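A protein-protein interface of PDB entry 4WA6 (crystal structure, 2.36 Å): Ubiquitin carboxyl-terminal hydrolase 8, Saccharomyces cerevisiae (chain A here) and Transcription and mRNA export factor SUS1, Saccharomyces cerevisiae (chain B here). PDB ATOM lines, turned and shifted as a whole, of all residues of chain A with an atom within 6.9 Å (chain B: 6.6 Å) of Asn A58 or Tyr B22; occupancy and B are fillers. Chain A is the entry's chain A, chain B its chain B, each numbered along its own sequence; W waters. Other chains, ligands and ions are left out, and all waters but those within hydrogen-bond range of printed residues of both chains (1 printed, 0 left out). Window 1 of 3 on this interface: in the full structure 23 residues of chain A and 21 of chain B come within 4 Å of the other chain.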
ATOM      1  N   PHE A  45     -18.086 -14.341 -18.535  1.00  0.00           N
ATOM      2  CA  PHE A  45     -16.704 -14.097 -18.185  1.00  0.00           C
ATOM      3  C   PHE A  45     -16.577 -13.663 -16.722  1.00  0.00           C
ATOM      4  O   PHE A  45     -15.752 -14.168 -15.996  1.00  0.00           O
ATOM      5  CB  PHE A  45     -16.075 -13.032 -19.079  1.00  0.00           C
ATOM      6  CG  PHE A  45     -15.780 -13.511 -20.451  1.00  0.00           C
ATOM      7  CD1 PHE A  45     -15.018 -14.658 -20.649  1.00  0.00           C
ATOM      8  CD2 PHE A  45     -16.279 -12.850 -21.537  1.00  0.00           C
ATOM      9  CE1 PHE A  45     -14.721 -15.107 -21.918  1.00  0.00           C
ATOM     10  CE2 PHE A  45     -16.007 -13.298 -22.818  1.00  0.00           C
ATOM     11  CZ  PHE A  45     -15.234 -14.432 -23.008  1.00  0.00           C
ATOM     12  N   THR A  48     -18.854 -16.504 -14.103  1.00  0.00           N
ATOM     13  CA  THR A  48     -18.561 -17.945 -14.120  1.00  0.00           C
ATOM     14  C   THR A  48     -17.170 -18.246 -14.602  1.00  0.00           C
ATOM     15  O   THR A  48     -16.771 -19.392 -14.582  1.00  0.00           O
ATOM     16  CB  THR A  48     -19.504 -18.769 -15.015  1.00  0.00           C
ATOM     17  OG1 THR A  48     -19.197 -18.494 -16.365  1.00  0.00           O
ATOM     18  CG2 THR A  48     -20.949 -18.429 -14.761  1.00  0.00           C
ATOM     19  N   MET A  49     -16.423 -17.243 -15.025  1.00  0.00           N
ATOM     20  CA  MET A  49     -15.073 -17.515 -15.498  1.00  0.00           C
ATOM     21  C   MET A  49     -14.033 -16.738 -14.754  1.00  0.00           C
ATOM     22  O   MET A  49     -12.917 -16.598 -15.199  1.00  0.00           O
ATOM     23  CB  MET A  49     -15.023 -17.298 -17.010  1.00  0.00           C
ATOM     24  CG  MET A  49     -15.693 -18.490 -17.709  1.00  0.00           C
ATOM     25  SD  MET A  49     -15.803 -18.293 -19.485  1.00  0.00           S
ATOM     26  CE  MET A  49     -16.611 -19.846 -19.882  1.00  0.00           C
ATOM     27  N   LYS A  50     -14.409 -16.267 -13.574  1.00  0.00           N
ATOM     28  CA  LYS A  50     -13.517 -15.489 -12.773  1.00  0.00           C
ATOM     29  C   LYS A  50     -13.239 -16.204 -11.473  1.00  0.00           C
ATOM     30  O   LYS A  50     -14.147 -16.541 -10.754  1.00  0.00           O
ATOM     31  CB  LYS A  50     -14.148 -14.140 -12.489  1.00  0.00           C
ATOM     32  CG  LYS A  50     -13.174 -13.184 -11.827  1.00  0.00           C
ATOM     33  CD  LYS A  50     -13.880 -12.265 -10.879  1.00  0.00           C
ATOM     34  CE  LYS A  50     -14.432 -11.064 -11.583  1.00  0.00           C
ATOM     35  NZ  LYS A  50     -14.595 -10.025 -10.529  1.00  0.00           N
ATOM     36  N   CYS A  51     -11.963 -16.397 -11.156  1.00  0.00           N
ATOM     37  CA  CYS A  51     -11.588 -17.050  -9.945  1.00  0.00           C
ATOM     38  C   CYS A  51     -11.868 -16.221  -8.706  1.00  0.00           C
ATOM     39  O   CYS A  51     -11.470 -15.068  -8.609  1.00  0.00           O
ATOM     40  CB  CYS A  51     -10.111 -17.384  -9.978  1.00  0.00           C
ATOM     41  SG  CYS A  51      -9.584 -18.393  -8.576  1.00  0.00           S
ATOM     42  N   GLU A  56      -8.594 -13.592 -11.626  1.00  0.00           N
ATOM     43  CA  GLU A  56      -8.300 -13.606 -13.049  1.00  0.00           C
ATOM     44  C   GLU A  56      -9.438 -14.249 -13.804  1.00  0.00           C
ATOM     45  O   GLU A  56     -10.063 -15.161 -13.299  1.00  0.00           O
ATOM     46  CB  GLU A  56      -7.019 -14.370 -13.348  1.00  0.00           C
ATOM     47  CG  GLU A  56      -5.770 -13.792 -12.703  1.00  0.00           C
ATOM     48  CD  GLU A  56      -4.501 -14.306 -13.355  1.00  0.00           C
ATOM     49  OE1 GLU A  56      -3.601 -14.795 -12.628  1.00  0.00           O
ATOM     50  OE2 GLU A  56      -4.409 -14.209 -14.604  1.00  0.00           O
ATOM     51  N   ILE A  57      -9.680 -13.756 -15.019  1.00  0.00           N
ATOM     52  CA  ILE A  57     -10.571 -14.375 -15.966  1.00  0.00           C
ATOM     53  C   ILE A  57      -9.862 -15.487 -16.767  1.00  0.00           C
ATOM     54  O   ILE A  57      -8.772 -15.273 -17.267  1.00  0.00           O
ATOM     55  CB  ILE A  57     -11.093 -13.345 -16.955  1.00  0.00           C
ATOM     56  CG1 ILE A  57     -11.574 -12.070 -16.223  1.00  0.00           C
ATOM     57  CG2 ILE A  57     -12.228 -13.945 -17.740  1.00  0.00           C
ATOM     58  CD1 ILE A  57     -12.777 -12.285 -15.351  1.00  0.00           C
ATOM     59  N   ASN A  58     -10.496 -16.654 -16.906  1.00  0.00           N
ATOM     60  CA  ASN A  58      -9.944 -17.769 -17.657  1.00  0.00           C
ATOM     61  C   ASN A  58      -8.536 -18.174 -17.244  1.00  0.00           C
ATOM     62  O   ASN A  58      -7.660 -18.297 -18.103  1.00  0.00           O
ATOM     63  CB  ASN A  58      -9.944 -17.436 -19.171  1.00  0.00           C
ATOM     64  CG  ASN A  58     -11.335 -17.372 -19.775  1.00  0.00           C
ATOM     65  OD1 ASN A  58     -12.243 -18.123 -19.415  1.00  0.00           O
ATOM     66  ND2 ASN A  58     -11.497 -16.504 -20.719  1.00  0.00           N
ATOM     67  N   SER A  59      -8.292 -18.393 -15.945  1.00  0.00           N
ATOM     68  CA  SER A  59      -6.984 -18.951 -15.432  1.00  0.00           C
ATOM     69  C   SER A  59      -7.034 -20.481 -15.542  1.00  0.00           C
ATOM     70  O   SER A  59      -7.125 -21.272 -14.553  1.00  0.00           O
ATOM     71  CB  SER A  59      -6.771 -18.512 -14.016  1.00  0.00           C
ATOM     72  OG  SER A  59      -5.494 -18.884 -13.552  1.00  0.00           O
ATOM     73  N   GLY A  60      -7.027 -20.888 -16.805  1.00  0.00           N
ATOM     74  CA  GLY A  60      -7.456 -22.190 -17.172  1.00  0.00           C
ATOM     75  C   GLY A  60      -8.948 -22.252 -16.947  1.00  0.00           C
ATOM     76  O   GLY A  60      -9.638 -21.212 -16.779  1.00  0.00           O
ATOM     77  N   ALA A  61      -9.444 -23.485 -16.963  1.00  0.00           N
ATOM     78  CA  ALA A  61     -10.821 -23.743 -16.678  1.00  0.00           C
ATOM     79  C   ALA A  61     -11.179 -23.159 -15.290  1.00  0.00           C
ATOM     80  O   ALA A  61     -10.382 -23.247 -14.343  1.00  0.00           O
ATOM     81  CB  ALA A  61     -11.061 -25.248 -16.711  1.00  0.00           C
ATOM     82  N   THR A  62     -12.377 -22.565 -15.175  1.00  0.00           N
ATOM     83  CA  THR A  62     -12.935 -22.115 -13.873  1.00  0.00           C
ATOM     84  C   THR A  62     -14.056 -23.042 -13.524  1.00  0.00           C
ATOM     85  O   THR A  62     -14.844 -23.422 -14.415  1.00  0.00           O
ATOM     86  CB  THR A  62     -13.421 -20.672 -13.953  1.00  0.00           C
ATOM     87  OG1 THR A  62     -12.375 -19.847 -14.490  1.00  0.00           O
ATOM     88  CG2 THR A  62     -13.818 -20.166 -12.617  1.00  0.00           C
ATOM     89  N   CYS A  73     -10.265 -21.327 -10.137  1.00  0.00           N
ATOM     90  CA  CYS A  73      -9.542 -21.642 -11.365  1.00  0.00           C
ATOM     91  C   CYS A  73      -8.737 -22.956 -11.294  1.00  0.00           C
ATOM     92  O   CYS A  73      -8.486 -23.482 -10.238  1.00  0.00           O
ATOM     93  CB  CYS A  73      -8.620 -20.485 -11.729  1.00  0.00           C
ATOM     94  SG  CYS A  73      -7.099 -20.250 -10.730  1.00  0.00           S
ATOM     95  N   ASN A  75      -5.491 -23.191 -13.213  1.00  0.00           N
ATOM     96  CA  ASN A  75      -4.075 -22.905 -13.314  1.00  0.00           C
ATOM     97  C   ASN A  75      -3.321 -22.641 -11.996  1.00  0.00           C
ATOM     98  O   ASN A  75      -2.145 -22.920 -11.914  1.00  0.00           O
ATOM     99  CB  ASN A  75      -3.833 -21.792 -14.338  1.00  0.00           C
ATOM    100  CG  ASN A  75      -4.084 -22.260 -15.770  1.00  0.00           C
ATOM    101  OD1 ASN A  75      -4.559 -23.341 -16.004  1.00  0.00           O
ATOM    102  ND2 ASN A  75      -3.795 -21.458 -16.703  1.00  0.00           N
ATOM    103  N   SER A  94     -17.078 -24.362 -16.337  1.00  0.00           N
ATOM    104  CA  SER A  94     -17.979 -23.354 -16.919  1.00  0.00           C
ATOM    105  C   SER A  94     -17.867 -23.165 -18.448  1.00  0.00           C
ATOM    106  O   SER A  94     -18.687 -22.444 -19.047  1.00  0.00           O
ATOM    107  CB  SER A  94     -17.860 -21.983 -16.210  1.00  0.00           C
ATOM    108  OG  SER A  94     -16.507 -21.544 -16.202  1.00  0.00           O
ATOM    109  N   ASN A  95     -16.870 -23.771 -19.078  1.00  0.00           N
ATOM    110  CA  ASN A  95     -16.809 -23.853 -20.542  1.00  0.00           C
ATOM    111  C   ASN A  95     -17.647 -24.977 -21.083  1.00  0.00           C
ATOM    112  O   ASN A  95     -17.988 -25.006 -22.245  1.00  0.00           O
ATOM    113  CB  ASN A  95     -15.411 -24.179 -20.998  1.00  0.00           C
ATOM    114  CG  ASN A  95     -14.434 -23.071 -20.738  1.00  0.00           C
ATOM    115  OD1 ASN A  95     -13.603 -23.167 -19.862  1.00  0.00           O
ATOM    116  ND2 ASN A  95     -14.580 -21.988 -21.448  1.00  0.00           N
ATOM    117  N   GLN B  13      -8.095  -7.119 -16.896  1.00  0.00           N
ATOM    118  CA  GLN B  13      -8.873  -8.172 -17.556  1.00  0.00           C
ATOM    119  C   GLN B  13     -10.348  -7.777 -17.571  1.00  0.00           C
ATOM    120  O   GLN B  13     -11.052  -7.859 -18.579  1.00  0.00           O
ATOM    121  CB  GLN B  13      -8.654  -9.503 -16.837  1.00  0.00           C
ATOM    122  CG  GLN B  13      -7.277 -10.087 -17.103  1.00  0.00           C
ATOM    123  CD  GLN B  13      -6.985 -11.366 -16.325  1.00  0.00           C
ATOM    124  OE1 GLN B  13      -7.849 -11.901 -15.683  1.00  0.00           O
ATOM    125  NE2 GLN B  13      -5.732 -11.816 -16.346  1.00  0.00           N
ATOM    126  N   TYR B  15     -11.611  -4.671 -17.391  1.00  0.00           N
ATOM    127  CA  TYR B  15     -11.933  -3.595 -18.344  1.00  0.00           C
ATOM    128  C   TYR B  15     -11.996  -4.129 -19.788  1.00  0.00           C
ATOM    129  O   TYR B  15     -12.904  -3.770 -20.579  1.00  0.00           O
ATOM    130  CB  TYR B  15     -10.970  -2.433 -18.241  1.00  0.00           C
ATOM    131  CG  TYR B  15     -11.305  -1.508 -17.111  1.00  0.00           C
ATOM    132  CD1 TYR B  15     -12.233  -0.486 -17.267  1.00  0.00           C
ATOM    133  CD2 TYR B  15     -10.660  -1.618 -15.891  1.00  0.00           C
ATOM    134  CE1 TYR B  15     -12.525   0.375 -16.216  1.00  0.00           C
ATOM    135  CE2 TYR B  15     -10.961  -0.785 -14.832  1.00  0.00           C
ATOM    136  CZ  TYR B  15     -11.879   0.205 -14.992  1.00  0.00           C
ATOM    137  OH  TYR B  15     -12.125   1.018 -13.912  1.00  0.00           O
ATOM    138  N   LEU B  16     -11.070  -5.026 -20.104  1.00  0.00           N
ATOM    139  CA  LEU B  16     -11.077  -5.716 -21.394  1.00  0.00           C
ATOM    140  C   LEU B  16     -12.414  -6.321 -21.668  1.00  0.00           C
ATOM    141  O   LEU B  16     -12.945  -6.174 -22.766  1.00  0.00           O
ATOM    142  CB  LEU B  16     -10.025  -6.800 -21.433  1.00  0.00           C
ATOM    143  CG  LEU B  16      -8.631  -6.414 -21.920  1.00  0.00           C
ATOM    144  CD1 LEU B  16      -7.730  -7.655 -21.908  1.00  0.00           C
ATOM    145  CD2 LEU B  16      -8.681  -5.818 -23.317  1.00  0.00           C
ATOM    146  N   VAL B  17     -12.979  -6.967 -20.654  1.00  0.00           N
ATOM    147  CA  VAL B  17     -14.267  -7.623 -20.790  1.00  0.00           C
ATOM    148  C   VAL B  17     -15.415  -6.632 -20.989  1.00  0.00           C
ATOM    149  O   VAL B  17     -16.256  -6.809 -21.867  1.00  0.00           O
ATOM    150  CB  VAL B  17     -14.555  -8.583 -19.602  1.00  0.00           C
ATOM    151  CG1 VAL B  17     -15.912  -9.236 -19.771  1.00  0.00           C
ATOM    152  CG2 VAL B  17     -13.505  -9.694 -19.533  1.00  0.00           C
ATOM    153  N   GLU B  18     -15.432  -5.571 -20.200  1.00  0.00           N
ATOM    154  CA  GLU B  18     -16.499  -4.551 -20.285  1.00  0.00           C
ATOM    155  C   GLU B  18     -16.513  -3.739 -21.580  1.00  0.00           C
ATOM    156  O   GLU B  18     -17.587  -3.336 -22.009  1.00  0.00           O
ATOM    157  CB  GLU B  18     -16.461  -3.614 -19.080  1.00  0.00           C
ATOM    158  CG  GLU B  18     -16.461  -4.355 -17.754  1.00  0.00           C
ATOM    159  CD  GLU B  18     -17.737  -4.208 -16.974  1.00  0.00           C
ATOM    160  OE1 GLU B  18     -18.817  -3.942 -17.562  1.00  0.00           O
ATOM    161  OE2 GLU B  18     -17.654  -4.335 -15.741  1.00  0.00           O
ATOM    162  N   SER B  19     -15.352  -3.487 -22.193  1.00  0.00           N
ATOM    163  CA  SER B  19     -15.310  -2.868 -23.536  1.00  0.00           C
ATOM    164  C   SER B  19     -15.955  -3.762 -24.635  1.00  0.00           C
ATOM    165  O   SER B  19     -16.533  -3.279 -25.554  1.00  0.00           O
ATOM    166  CB  SER B  19     -13.872  -2.484 -23.928  1.00  0.00           C
ATOM    167  OG  SER B  19     -12.976  -3.602 -23.950  1.00  0.00           O
ATOM    168  N   GLY B  20     -15.873  -5.075 -24.503  1.00  0.00           N
ATOM    169  CA  GLY B  20     -16.264  -5.989 -25.569  1.00  0.00           C
ATOM    170  C   GLY B  20     -15.000  -6.546 -26.211  1.00  0.00           C
ATOM    171  O   GLY B  20     -15.064  -7.508 -26.982  1.00  0.00           O
ATOM    172  N   ASN B  21     -13.849  -5.967 -25.885  1.00  0.00           N
ATOM    173  CA  ASN B  21     -12.609  -6.342 -26.562  1.00  0.00           C
ATOM    174  C   ASN B  21     -12.060  -7.686 -26.178  1.00  0.00           C
ATOM    175  O   ASN B  21     -11.327  -8.289 -26.961  1.00  0.00           O
ATOM    176  CB  ASN B  21     -11.533  -5.264 -26.390  1.00  0.00           C
ATOM    177  CG  ASN B  21     -11.949  -3.930 -27.022  1.00  0.00           C
ATOM    178  OD1 ASN B  21     -12.711  -3.923 -27.994  1.00  0.00           O
ATOM    179  ND2 ASN B  21     -11.451  -2.816 -26.486  1.00  0.00           N
ATOM    180  N   TYR B  22     -12.429  -8.187 -24.999  1.00  0.00           N
ATOM    181  CA  TYR B  22     -12.039  -9.573 -24.593  1.00  0.00           C
ATOM    182  C   TYR B  22     -12.720 -10.567 -25.489  1.00  0.00           C
ATOM    183  O   TYR B  22     -12.116 -11.529 -25.929  1.00  0.00           O
ATOM    184  CB  TYR B  22     -12.415  -9.840 -23.130  1.00  0.00           C
ATOM    185  CG  TYR B  22     -11.737 -11.043 -22.529  1.00  0.00           C
ATOM    186  CD1 TYR B  22     -10.467 -10.938 -21.974  1.00  0.00           C
ATOM    187  CD2 TYR B  22     -12.368 -12.263 -22.475  1.00  0.00           C
ATOM    188  CE1 TYR B  22      -9.812 -12.044 -21.403  1.00  0.00           C
ATOM    189  CE2 TYR B  22     -11.731 -13.375 -21.938  1.00  0.00           C
ATOM    190  CZ  TYR B  22     -10.458 -13.263 -21.386  1.00  0.00           C
ATOM    191  OH  TYR B  22      -9.836 -14.322 -20.787  1.00  0.00           O
ATOM    192  N   GLU B  23     -13.994 -10.352 -25.752  1.00  0.00           N
ATOM    193  CA  GLU B  23     -14.694 -11.173 -26.747  1.00  0.00           C
ATOM    194  C   GLU B  23     -14.081 -11.110 -28.140  1.00  0.00           C
ATOM    195  O   GLU B  23     -14.071 -12.105 -28.855  1.00  0.00           O
ATOM    196  CB  GLU B  23     -16.131 -10.733 -26.912  1.00  0.00           C
ATOM    197  CG  GLU B  23     -17.078 -11.212 -25.840  1.00  0.00           C
ATOM    198  CD  GLU B  23     -18.338 -10.360 -25.862  1.00  0.00           C
ATOM    199  OE1 GLU B  23     -19.267 -10.804 -26.589  1.00  0.00           O
ATOM    200  OE2 GLU B  23     -18.359  -9.243 -25.225  1.00  0.00           O
ATOM    201  N   LEU B  24     -13.677  -9.925 -28.571  1.00  0.00           N
ATOM    202  CA  LEU B  24     -13.123  -9.820 -29.910  1.00  0.00           C
ATOM    203  C   LEU B  24     -11.833 -10.646 -29.954  1.00  0.00           C
ATOM    204  O   LEU B  24     -11.643 -11.443 -30.851  1.00  0.00           O
ATOM    205  CB  LEU B  24     -12.844  -8.357 -30.308  1.00  0.00           C
ATOM    206  CG  LEU B  24     -14.042  -7.446 -30.581  1.00  0.00           C
ATOM    207  CD1 LEU B  24     -13.603  -5.992 -30.733  1.00  0.00           C
ATOM    208  CD2 LEU B  24     -14.812  -7.877 -31.821  1.00  0.00           C
ATOM    209  N   ILE B  25     -10.969 -10.474 -28.960  1.00  0.00           N
ATOM    210  CA  ILE B  25      -9.664 -11.115 -28.945  1.00  0.00           C
ATOM    211  C   ILE B  25      -9.876 -12.607 -28.935  1.00  0.00           C
ATOM    212  O   ILE B  25      -9.260 -13.356 -29.685  1.00  0.00           O
ATOM    213  CB  ILE B  25      -8.892 -10.721 -27.677  1.00  0.00           C
ATOM    214  CG1 ILE B  25      -8.405  -9.269 -27.776  1.00  0.00           C
ATOM    215  CG2 ILE B  25      -7.711 -11.671 -27.448  1.00  0.00           C
ATOM    216  CD1 ILE B  25      -8.102  -8.637 -26.433  1.00  0.00           C
ATOM    217  N   SER B  26     -10.783 -13.033 -28.077  1.00  0.00           N
ATOM    218  CA  SER B  26     -11.047 -14.439 -27.920  1.00  0.00           C
ATOM    219  C   SER B  26     -11.698 -15.031 -29.153  1.00  0.00           C
ATOM    220  O   SER B  26     -11.364 -16.123 -29.592  1.00  0.00           O
ATOM    221  CB  SER B  26     -11.927 -14.638 -26.705  1.00  0.00           C
ATOM    222  OG  SER B  26     -12.407 -15.926 -26.703  1.00  0.00           O
ATOM    223  N   ASN B  27     -12.552 -14.260 -29.801  1.00  0.00           N
ATOM    224  CA  ASN B  27     -13.103 -14.743 -31.042  1.00  0.00           C
ATOM    225  C   ASN B  27     -12.119 -14.780 -32.175  1.00  0.00           C
ATOM    226  O   ASN B  27     -12.185 -15.639 -33.027  1.00  0.00           O
ATOM    227  CB  ASN B  27     -14.352 -13.965 -31.398  1.00  0.00           C
ATOM    228  CG  ASN B  27     -15.482 -14.315 -30.484  1.00  0.00           C
ATOM    229  OD1 ASN B  27     -15.595 -15.447 -30.019  1.00  0.00           O
ATOM    230  ND2 ASN B  27     -16.279 -13.357 -30.182  1.00  0.00           N
ATOM    231  N   PHE B  88      -4.977  -3.040 -27.247  1.00  0.00           N
ATOM    232  CA  PHE B  88      -6.074  -2.810 -26.338  1.00  0.00           C
ATOM    233  C   PHE B  88      -5.600  -2.427 -24.935  1.00  0.00           C
ATOM    234  O   PHE B  88      -6.189  -1.553 -24.296  1.00  0.00           O
ATOM    235  CB  PHE B  88      -6.982  -4.047 -26.254  1.00  0.00           C
ATOM    236  CG  PHE B  88      -7.823  -4.300 -27.495  1.00  0.00           C
ATOM    237  CD1 PHE B  88      -8.556  -3.287 -28.084  1.00  0.00           C
ATOM    238  CD2 PHE B  88      -7.940  -5.572 -28.017  1.00  0.00           C
ATOM    239  CE1 PHE B  88      -9.343  -3.529 -29.204  1.00  0.00           C
ATOM    240  CE2 PHE B  88      -8.738  -5.829 -29.119  1.00  0.00           C
ATOM    241  CZ  PHE B  88      -9.430  -4.800 -29.726  1.00  0.00           C
HETATM  242  O   HOH W   1      -7.672 -13.360 -18.901  1.00  0.00           O
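The backbone NH (N) of Ile A57 is in hydrogen-bond range of the side-chain amide oxygen (OE1) of Gln B13. The side-chain amide nitrogen (NE2) of Gln B13 is in hydrogen-bond range of the side-chain carboxylate (OE2) of Glu A56 (3.2 Å). The side-chain amide nitrogen (ND2) of Asn A58 lies within hydrogen-bond range of the side-chain hydroxyl (OH) of Tyr B22 (2.7 Å).
The backbone carbonyl oxygen (O) of Leu B16 lies within hydrogen-bond range of the backbone NH (N) of Tyr B22, at 3.1 Å. The backbone carbonyl oxygen of Glu B23 sits at hydrogen-bond distance from the side-chain amide nitrogen of Asn B27 (2.9 Å). The backbone NH (N) of Asn A58 is in hydrogen-bond range of the backbone carbonyl oxygen (O) of Met A49. The backbone carbonyl oxygen (O) of Glu A56 lies within hydrogen-bond range of the backbone NH (N) of Cys A51, at 3.1 Å. N of Lys A50 is in hydrogen-bond range of O of Phe A45 (3.5 Å).
Phe A45 touches Val B17 (CB to CG1, 3.9 Å). Phe A45 touches Tyr B22 (CE1 to CE2, 3.5 Å). CE2 of Phe A45 touches CG of Glu B23, at 3.8 Å. Ile A57 touches Tyr B22.
Asn A58 touches just one residue of chain B: Tyr B22 (2.7 Å). Tyr B22 touches three residues of chain A. Printed residues of chain A within 4 Å of Gln B13: Glu A56 (3.2 Å) and Ile A57 (2.7 Å). Of the printed residues of chain B, Glu A56 touches Gln B13 (3.2 Å). Printed residues of chain B within 4 Å of Ile A57: Gln B13 and Tyr B22. Printed residues of chain B within 4 Å of Phe A45: Val B17, Tyr B22 and Glu B23. Lys A50 touches none of the printed residues of chain B. Gly A60 touches none of the printed residues of chain B. The nearest residue of chain B that does not touch Asn A58 is Gln B13 (5.6 Å). The nearest residue of chain A that does not touch Tyr B22 is Ser A59 (6.5 Å).
Hydrophobic or aromatic side chains of chain B within 4 Å of the printed part of chain A: Val B17 and Tyr B22. Of the 16 printed residues of chain A, 4 touch a printed residue of chain B. Hydrophobic or aromatic side chains of chain A within 4 Å of the printed part of chain B: Phe A45 and Ile A57. Among the printed residues, 7 pairs touch across the chains.
Water W1 bridges the backbone carbonyl oxygen of Ile A57 (2.7 Å) and the side-chain hydroxyl of Tyr B22 (3.0 Å).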
